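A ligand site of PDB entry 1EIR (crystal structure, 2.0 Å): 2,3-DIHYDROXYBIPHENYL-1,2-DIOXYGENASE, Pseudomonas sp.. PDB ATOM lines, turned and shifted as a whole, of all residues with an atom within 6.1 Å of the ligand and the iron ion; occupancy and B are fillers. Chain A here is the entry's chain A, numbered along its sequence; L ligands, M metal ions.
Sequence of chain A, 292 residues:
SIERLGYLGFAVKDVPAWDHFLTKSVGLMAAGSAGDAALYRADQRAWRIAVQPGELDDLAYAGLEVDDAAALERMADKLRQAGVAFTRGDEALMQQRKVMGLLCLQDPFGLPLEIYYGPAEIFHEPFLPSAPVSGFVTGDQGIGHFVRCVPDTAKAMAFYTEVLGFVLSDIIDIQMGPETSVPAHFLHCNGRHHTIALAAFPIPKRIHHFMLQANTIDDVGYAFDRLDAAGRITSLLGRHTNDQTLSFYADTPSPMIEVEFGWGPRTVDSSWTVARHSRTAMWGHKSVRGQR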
ATOM      1  N   HIS A 145      20.811  15.094  32.092  1.00  0.00           N
ATOM      2  CA  HIS A 145      21.677  13.923  32.103  1.00  0.00           C
ATOM      3  C   HIS A 145      23.146  14.324  32.297  1.00  0.00           C
ATOM      4  O   HIS A 145      23.482  15.522  32.315  1.00  0.00           O
ATOM      5  CB  HIS A 145      21.543  13.136  30.797  1.00  0.00           C
ATOM      6  CG  HIS A 145      22.287  13.735  29.635  1.00  0.00           C
ATOM      7  ND1 HIS A 145      21.641  14.323  28.563  1.00  0.00           N
ATOM      8  CD2 HIS A 145      23.608  13.823  29.371  1.00  0.00           C
ATOM      9  CE1 HIS A 145      22.542  14.740  27.698  1.00  0.00           C
ATOM     10  NE2 HIS A 145      23.740  14.453  28.165  1.00  0.00           N
ATOM     11  N   VAL A 147      27.400  12.576  31.619  1.00  0.00           N
ATOM     12  CA  VAL A 147      28.254  11.497  31.137  1.00  0.00           C
ATOM     13  C   VAL A 147      29.260  11.110  32.222  1.00  0.00           C
ATOM     14  O   VAL A 147      30.096  11.918  32.621  1.00  0.00           O
ATOM     15  CB  VAL A 147      29.012  11.924  29.857  1.00  0.00           C
ATOM     16  CG1 VAL A 147      29.974  10.832  29.445  1.00  0.00           C
ATOM     17  CG2 VAL A 147      28.019  12.219  28.738  1.00  0.00           C
ATOM     18  N   ILE A 172      27.493   4.675  21.015  1.00  0.00           N
ATOM     19  CA  ILE A 172      28.147   5.496  20.006  1.00  0.00           C
ATOM     20  C   ILE A 172      29.636   5.286  20.173  1.00  0.00           C
ATOM     21  O   ILE A 172      30.161   5.368  21.290  1.00  0.00           O
ATOM     22  CB  ILE A 172      27.854   7.007  20.155  1.00  0.00           C
ATOM     23  CG1 ILE A 172      26.346   7.275  20.009  1.00  0.00           C
ATOM     24  CG2 ILE A 172      28.616   7.791  19.064  1.00  0.00           C
ATOM     25  CD1 ILE A 172      25.980   8.744  20.067  1.00  0.00           C
ATOM     26  N   ILE A 174      32.701   6.833  19.967  1.00  0.00           N
ATOM     27  CA  ILE A 174      33.264   8.165  19.893  1.00  0.00           C
ATOM     28  C   ILE A 174      34.740   8.076  19.539  1.00  0.00           C
ATOM     29  O   ILE A 174      35.534   7.548  20.305  1.00  0.00           O
ATOM     30  CB  ILE A 174      33.081   8.914  21.231  1.00  0.00           C
ATOM     31  CG1 ILE A 174      31.582   9.003  21.557  1.00  0.00           C
ATOM     32  CG2 ILE A 174      33.696  10.297  21.139  1.00  0.00           C
ATOM     33  CD1 ILE A 174      31.272   9.441  22.974  1.00  0.00           C
ATOM     34  N   ALA A 184      30.724   4.657  23.969  1.00  0.00           N
ATOM     35  CA  ALA A 184      29.922   5.329  24.986  1.00  0.00           C
ATOM     36  C   ALA A 184      28.562   4.666  25.076  1.00  0.00           C
ATOM     37  O   ALA A 184      27.887   4.522  24.056  1.00  0.00           O
ATOM     38  CB  ALA A 184      29.751   6.795  24.624  1.00  0.00           C
ATOM     39  N   PHE A 186      24.749   4.806  26.392  1.00  0.00           N
ATOM     40  CA  PHE A 186      23.697   5.702  26.858  1.00  0.00           C
ATOM     41  C   PHE A 186      22.561   4.926  27.511  1.00  0.00           C
ATOM     42  O   PHE A 186      22.019   3.982  26.935  1.00  0.00           O
ATOM     43  CB  PHE A 186      23.203   6.557  25.687  1.00  0.00           C
ATOM     44  CG  PHE A 186      24.292   7.384  25.056  1.00  0.00           C
ATOM     45  CD1 PHE A 186      25.194   6.803  24.176  1.00  0.00           C
ATOM     46  CD2 PHE A 186      24.455   8.721  25.412  1.00  0.00           C
ATOM     47  CE1 PHE A 186      26.265   7.543  23.664  1.00  0.00           C
ATOM     48  CE2 PHE A 186      25.518   9.463  24.906  1.00  0.00           C
ATOM     49  CZ  PHE A 186      26.423   8.874  24.032  1.00  0.00           C
ATOM     50  N   HIS A 193      15.888  10.255  26.425  1.00  0.00           N
ATOM     51  CA  HIS A 193      16.717   9.301  25.695  1.00  0.00           C
ATOM     52  C   HIS A 193      17.788   8.700  26.595  1.00  0.00           C
ATOM     53  O   HIS A 193      18.001   7.490  26.601  1.00  0.00           O
ATOM     54  CB  HIS A 193      17.384   9.939  24.475  1.00  0.00           C
ATOM     55  CG  HIS A 193      18.319   9.004  23.770  1.00  0.00           C
ATOM     56  ND1 HIS A 193      19.673   9.002  23.993  1.00  0.00           N
ATOM     57  CD2 HIS A 193      18.080   7.993  22.893  1.00  0.00           C
ATOM     58  CE1 HIS A 193      20.233   8.025  23.298  1.00  0.00           C
ATOM     59  NE2 HIS A 193      19.286   7.400  22.623  1.00  0.00           N
ATOM     60  N   HIS A 194      18.469   9.545  27.356  1.00  0.00           N
ATOM     61  CA  HIS A 194      19.458   9.056  28.310  1.00  0.00           C
ATOM     62  C   HIS A 194      19.623  10.022  29.466  1.00  0.00           C
ATOM     63  O   HIS A 194      19.588  11.250  29.284  1.00  0.00           O
ATOM     64  CB  HIS A 194      20.797   8.722  27.634  1.00  0.00           C
ATOM     65  CG  HIS A 194      21.484   9.899  27.009  1.00  0.00           C
ATOM     66  ND1 HIS A 194      22.566  10.524  27.590  1.00  0.00           N
ATOM     67  CD2 HIS A 194      21.258  10.540  25.833  1.00  0.00           C
ATOM     68  CE1 HIS A 194      22.981  11.499  26.802  1.00  0.00           C
ATOM     69  NE2 HIS A 194      22.206  11.528  25.730  1.00  0.00           N
ATOM     70  N   ALA A 197      25.215   8.397  30.823  1.00  0.00           N
ATOM     71  CA  ALA A 197      25.989   7.719  29.789  1.00  0.00           C
ATOM     72  C   ALA A 197      27.320   7.329  30.419  1.00  0.00           C
ATOM     73  O   ALA A 197      27.893   8.079  31.210  1.00  0.00           O
ATOM     74  CB  ALA A 197      26.204   8.641  28.586  1.00  0.00           C
ATOM     75  N   ALA A 199      31.266   6.105  29.675  1.00  0.00           N
ATOM     76  CA  ALA A 199      32.317   6.104  28.651  1.00  0.00           C
ATOM     77  C   ALA A 199      33.720   6.083  29.275  1.00  0.00           C
ATOM     78  O   ALA A 199      34.010   6.857  30.197  1.00  0.00           O
ATOM     79  CB  ALA A 199      32.173   7.334  27.745  1.00  0.00           C
ATOM     80  N   PHE A 201      36.618   7.452  29.088  1.00  0.00           N
ATOM     81  CA  PHE A 201      37.402   8.574  28.583  1.00  0.00           C
ATOM     82  C   PHE A 201      38.693   8.812  29.369  1.00  0.00           C
ATOM     83  O   PHE A 201      38.745   8.606  30.590  1.00  0.00           O
ATOM     84  CB  PHE A 201      36.590   9.867  28.644  1.00  0.00           C
ATOM     85  CG  PHE A 201      35.542   9.978  27.584  1.00  0.00           C
ATOM     86  CD1 PHE A 201      34.342  10.636  27.839  1.00  0.00           C
ATOM     87  CD2 PHE A 201      35.753   9.425  26.311  1.00  0.00           C
ATOM     88  CE1 PHE A 201      33.365  10.760  26.845  1.00  0.00           C
ATOM     89  CE2 PHE A 201      34.786   9.539  25.317  1.00  0.00           C
ATOM     90  CZ  PHE A 201      33.578  10.207  25.590  1.00  0.00           C
ATOM     91  N   HIS A 208      32.229  14.032  32.255  1.00  0.00           N
ATOM     92  CA  HIS A 208      32.700  14.772  31.101  1.00  0.00           C
ATOM     93  C   HIS A 208      31.884  16.056  31.000  1.00  0.00           C
ATOM     94  O   HIS A 208      32.398  17.116  30.638  1.00  0.00           O
ATOM     95  CB  HIS A 208      32.546  13.893  29.850  1.00  0.00           C
ATOM     96  CG  HIS A 208      32.867  14.601  28.574  1.00  0.00           C
ATOM     97  ND1 HIS A 208      31.938  15.381  27.913  1.00  0.00           N
ATOM     98  CD2 HIS A 208      34.001  14.670  27.850  1.00  0.00           C
ATOM     99  CE1 HIS A 208      32.500  15.899  26.832  1.00  0.00           C
ATOM    100  NE2 HIS A 208      33.754  15.478  26.769  1.00  0.00           N
ATOM    101  N   HIS A 209      30.595  15.964  31.319  1.00  0.00           N
ATOM    102  CA  HIS A 209      29.697  17.116  31.292  1.00  0.00           C
ATOM    103  C   HIS A 209      28.311  16.758  31.824  1.00  0.00           C
ATOM    104  O   HIS A 209      27.987  15.573  31.992  1.00  0.00           O
ATOM    105  CB  HIS A 209      29.566  17.647  29.851  1.00  0.00           C
ATOM    106  CG  HIS A 209      28.658  16.823  28.987  1.00  0.00           C
ATOM    107  ND1 HIS A 209      29.124  15.849  28.129  1.00  0.00           N
ATOM    108  CD2 HIS A 209      27.311  16.813  28.856  1.00  0.00           C
ATOM    109  CE1 HIS A 209      28.117  15.269  27.511  1.00  0.00           C
ATOM    110  NE2 HIS A 209      26.995  15.840  27.938  1.00  0.00           N
ATOM    111  N   PHE A 210      27.506  17.785  32.111  1.00  0.00           N
ATOM    112  CA  PHE A 210      26.131  17.582  32.540  1.00  0.00           C
ATOM    113  C   PHE A 210      25.296  18.366  31.527  1.00  0.00           C
ATOM    114  O   PHE A 210      25.769  19.347  30.967  1.00  0.00           O
ATOM    115  CB  PHE A 210      25.872  18.055  33.990  1.00  0.00           C
ATOM    116  CG  PHE A 210      25.860  19.554  34.177  1.00  0.00           C
ATOM    117  CD1 PHE A 210      24.652  20.249  34.266  1.00  0.00           C
ATOM    118  CD2 PHE A 210      27.051  20.261  34.317  1.00  0.00           C
ATOM    119  CE1 PHE A 210      24.629  21.616  34.500  1.00  0.00           C
ATOM    120  CE2 PHE A 210      27.048  21.637  34.556  1.00  0.00           C
ATOM    121  CZ  PHE A 210      25.829  22.321  34.651  1.00  0.00           C
ATOM    122  N   MET A 211      24.078  17.906  31.272  1.00  0.00           N
ATOM    123  CA  MET A 211      23.237  18.566  30.277  1.00  0.00           C
ATOM    124  C   MET A 211      21.895  19.097  30.788  1.00  0.00           C
ATOM    125  O   MET A 211      21.253  18.477  31.632  1.00  0.00           O
ATOM    126  CB  MET A 211      22.984  17.596  29.113  1.00  0.00           C
ATOM    127  CG  MET A 211      22.164  18.172  27.963  1.00  0.00           C
ATOM    128  SD  MET A 211      20.379  17.879  28.154  1.00  0.00           S
ATOM    129  CE  MET A 211      19.782  18.518  26.579  1.00  0.00           C
ATOM    130  N   HIS A 240      22.624  15.625  17.781  1.00  0.00           N
ATOM    131  CA  HIS A 240      23.159  14.289  18.009  1.00  0.00           C
ATOM    132  C   HIS A 240      22.510  13.224  17.122  1.00  0.00           C
ATOM    133  O   HIS A 240      21.397  13.390  16.622  1.00  0.00           O
ATOM    134  CB  HIS A 240      23.000  13.911  19.482  1.00  0.00           C
ATOM    135  CG  HIS A 240      23.919  14.663  20.401  1.00  0.00           C
ATOM    136  ND1 HIS A 240      25.285  14.563  20.318  1.00  0.00           N
ATOM    137  CD2 HIS A 240      23.660  15.526  21.400  1.00  0.00           C
ATOM    138  CE1 HIS A 240      25.837  15.331  21.238  1.00  0.00           C
ATOM    139  NE2 HIS A 240      24.866  15.923  21.919  1.00  0.00           N
ATOM    140  N   THR A 241      23.242  12.128  16.946  1.00  0.00           N
ATOM    141  CA  THR A 241      22.793  11.001  16.144  1.00  0.00           C
ATOM    142  C   THR A 241      21.758  10.148  16.881  1.00  0.00           C
ATOM    143  O   THR A 241      20.755   9.743  16.305  1.00  0.00           O
ATOM    144  CB  THR A 241      23.993  10.079  15.785  1.00  0.00           C
ATOM    145  OG1 THR A 241      24.755   9.786  16.961  1.00  0.00           O
ATOM    146  CG2 THR A 241      24.903  10.736  14.739  1.00  0.00           C
ATOM    147  N   ASN A 242      22.006   9.896  18.160  1.00  0.00           N
ATOM    148  CA  ASN A 242      21.105   9.067  18.955  1.00  0.00           C
ATOM    149  C   ASN A 242      19.881   9.737  19.594  1.00  0.00           C
ATOM    150  O   ASN A 242      18.755   9.270  19.386  1.00  0.00           O
ATOM    151  CB  ASN A 242      21.904   8.293  20.016  1.00  0.00           C
ATOM    152  CG  ASN A 242      22.649   9.207  20.991  1.00  0.00           C
ATOM    153  OD1 ASN A 242      22.732  10.429  20.809  1.00  0.00           O
ATOM    154  ND2 ASN A 242      23.195   8.606  22.044  1.00  0.00           N
ATOM    155  N   ASP A 243      20.056  10.815  20.355  1.00  0.00           N
ATOM    156  CA  ASP A 243      18.904  11.456  20.977  1.00  0.00           C
ATOM    157  C   ASP A 243      18.309  12.576  20.141  1.00  0.00           C
ATOM    158  O   ASP A 243      17.218  13.060  20.441  1.00  0.00           O
ATOM    159  CB  ASP A 243      19.237  11.973  22.389  1.00  0.00           C
ATOM    160  CG  ASP A 243      20.192  13.162  22.388  1.00  0.00           C
ATOM    161  OD1 ASP A 243      20.684  13.537  23.479  1.00  0.00           O
ATOM    162  OD2 ASP A 243      20.465  13.739  21.306  1.00  0.00           O
ATOM    163  N   THR A 245      19.188  15.567  19.955  1.00  0.00           N
ATOM    164  CA  THR A 245      19.166  16.801  20.715  1.00  0.00           C
ATOM    165  C   THR A 245      19.952  17.835  19.905  1.00  0.00           C
ATOM    166  O   THR A 245      20.978  17.520  19.309  1.00  0.00           O
ATOM    167  CB  THR A 245      19.838  16.618  22.097  1.00  0.00           C
ATOM    168  OG1 THR A 245      18.950  15.901  22.966  1.00  0.00           O
ATOM    169  CG2 THR A 245      20.159  17.981  22.731  1.00  0.00           C
ATOM    170  N   SER A 247      22.047  20.987  20.361  1.00  0.00           N
ATOM    171  CA  SER A 247      22.720  21.699  21.429  1.00  0.00           C
ATOM    172  C   SER A 247      24.104  22.215  21.065  1.00  0.00           C
ATOM    173  O   SER A 247      24.533  22.177  19.914  1.00  0.00           O
ATOM    174  CB  SER A 247      22.873  20.755  22.619  1.00  0.00           C
ATOM    175  OG  SER A 247      23.558  19.576  22.222  1.00  0.00           O
ATOM    176  N   TYR A 249      28.128  22.915  23.339  1.00  0.00           N
ATOM    177  CA  TYR A 249      28.842  22.649  24.577  1.00  0.00           C
ATOM    178  C   TYR A 249      29.638  23.874  24.996  1.00  0.00           C
ATOM    179  O   TYR A 249      29.938  24.745  24.169  1.00  0.00           O
ATOM    180  CB  TYR A 249      29.773  21.448  24.405  1.00  0.00           C
ATOM    181  CG  TYR A 249      29.044  20.130  24.193  1.00  0.00           C
ATOM    182  CD1 TYR A 249      28.964  19.187  25.215  1.00  0.00           C
ATOM    183  CD2 TYR A 249      28.484  19.803  22.956  1.00  0.00           C
ATOM    184  CE1 TYR A 249      28.362  17.948  25.017  1.00  0.00           C
ATOM    185  CE2 TYR A 249      27.885  18.578  22.742  1.00  0.00           C
ATOM    186  CZ  TYR A 249      27.823  17.652  23.764  1.00  0.00           C
ATOM    187  OH  TYR A 249      27.255  16.418  23.541  1.00  0.00           O
ATOM    188  N   GLU A 260      26.248  21.051  28.570  1.00  0.00           N
ATOM    189  CA  GLU A 260      25.575  20.981  27.287  1.00  0.00           C
ATOM    190  C   GLU A 260      24.192  21.601  27.462  1.00  0.00           C
ATOM    191  O   GLU A 260      23.451  21.289  28.388  1.00  0.00           O
ATOM    192  CB  GLU A 260      25.462  19.535  26.819  1.00  0.00           C
ATOM    193  CG  GLU A 260      24.991  19.416  25.379  1.00  0.00           C
ATOM    194  CD  GLU A 260      24.723  17.986  24.960  1.00  0.00           C
ATOM    195  OE1 GLU A 260      24.791  17.099  25.821  1.00  0.00           O
ATOM    196  OE2 GLU A 260      24.463  17.751  23.765  1.00  0.00           O
ATOM    197  N   THR A 280      28.801  11.104  17.005  1.00  0.00           N
ATOM    198  CA  THR A 280      27.954  11.662  18.071  1.00  0.00           C
ATOM    199  C   THR A 280      27.041  12.730  17.509  1.00  0.00           C
ATOM    200  O   THR A 280      26.077  13.129  18.152  1.00  0.00           O
ATOM    201  CB  THR A 280      28.777  12.312  19.228  1.00  0.00           C
ATOM    202  OG1 THR A 280      29.581  13.377  18.702  1.00  0.00           O
ATOM    203  CG2 THR A 280      29.643  11.283  19.945  1.00  0.00           C
HETATM  204  C1  LIG L   1      26.826  11.769  22.424  1.00  0.00           C
HETATM  205  C2  LIG L   1      27.174  12.690  23.494  1.00  0.00           C
HETATM  206  C3  LIG L   1      26.139  13.427  24.179  1.00  0.00           C
HETATM  207  C4  LIG L   1      24.751  13.244  23.817  1.00  0.00           C
HETATM  208  C5  LIG L   1      24.396  12.324  22.753  1.00  0.00           C
HETATM  209  C6  LIG L   1      25.435  11.594  22.057  1.00  0.00           C
HETATM  210  C7  LIG L   1      28.536  12.866  23.875  1.00  0.00           C
HETATM  211  C8  LIG L   1      29.030  12.268  25.104  1.00  0.00           C
HETATM  212  C9  LIG L   1      30.415  12.474  25.502  1.00  0.00           C
HETATM  213  C10 LIG L   1      31.297  13.279  24.677  1.00  0.00           C
HETATM  214  C11 LIG L   1      30.807  13.891  23.449  1.00  0.00           C
HETATM  215  C12 LIG L   1      29.430  13.683  23.045  1.00  0.00           C
HETATM  216  O1  LIG L   1      23.775  13.971  24.463  1.00  0.00           O
HETATM  217  O2  LIG L   1      26.471  14.311  25.178  1.00  0.00           O
HETATM  218 FE    FE M   1      25.276  15.033  26.506  1.00  0.00          FE
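Val 147 touches the ligand. Ile 172 touches the ligand (CD1 to C6, 3.5 Å). Phe 186 touches the ligand. CE1 of Phe 201 touches C9 of the ligand (3.7 Å). His 208 touches the ligand (CE1 to C10, 3.6 Å). Asn 242 touches the ligand (OD1 to C5, 3.2 Å). Thr 280 touches the ligand. Within 4 Å of the ligand: His 145, Val 147, Ile 172, Phe 186, His 194, Phe 201, His 208, His 209, His 240, Asn 242, Asp 243, Tyr 249, Glu 260 and Thr 280.
An oxygen (O2) of the ligand binds the iron ion (1.9 Å). The side-chain carboxylate (OE1) of Glu 260 binds the iron ion, 2.2 Å away. NE2 of His 145 binds the iron ion (2.3 Å). The iron ion is bound by a ring nitrogen (NE2) of His 209, 2.4 Å away. Slightly farther from the iron ion lies an oxygen (O1) of the ligand (2.7 Å).
Residues that only touch the iron ion: Tyr 249. Within 4 Å of the iron ion: His 145, His 209, Tyr 249 and Glu 260.
OH of Tyr 249 lies within hydrogen-bond range of OE2 of Glu 260, at 3.1 Å. OE2 of Glu 260 sits at hydrogen-bond distance from NE2 of His 240. OG of Ser 247 lies within hydrogen-bond range of OE2 of Glu 260 (2.6 Å). The backbone carbonyl oxygen (O) of His 145 sits at hydrogen-bond distance from the backbone NH (N) of Met 211. A ring nitrogen (ND1) of His 208 lies within hydrogen-bond range of a ring nitrogen (ND1) of His 209 (2.9 Å). OD1 of Asp 243 is in hydrogen-bond range of NE2 of His 194 (3.4 Å). The backbone NH (N) of Thr 245 sits at hydrogen-bond distance from the side-chain carboxylate (OD2) of Asp 243. ND1 of His 240 lies within hydrogen-bond range of O of Thr 280, at 2.7 Å.
An oxygen (O2) of the ligand sits close to the side-chain hydroxyl of Tyr 249. A ring nitrogen (NE2) of His 194 is in hydrogen-bond range of an oxygen (O1) of the ligand (3.2 Å). The side-chain carboxylate of Asp 243 sits at hydrogen-bond distance from an oxygen (O1) of the ligand. A ring nitrogen (NE2) of His 240 sits close to an oxygen (O1) of the ligand, 3.4 Å away.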
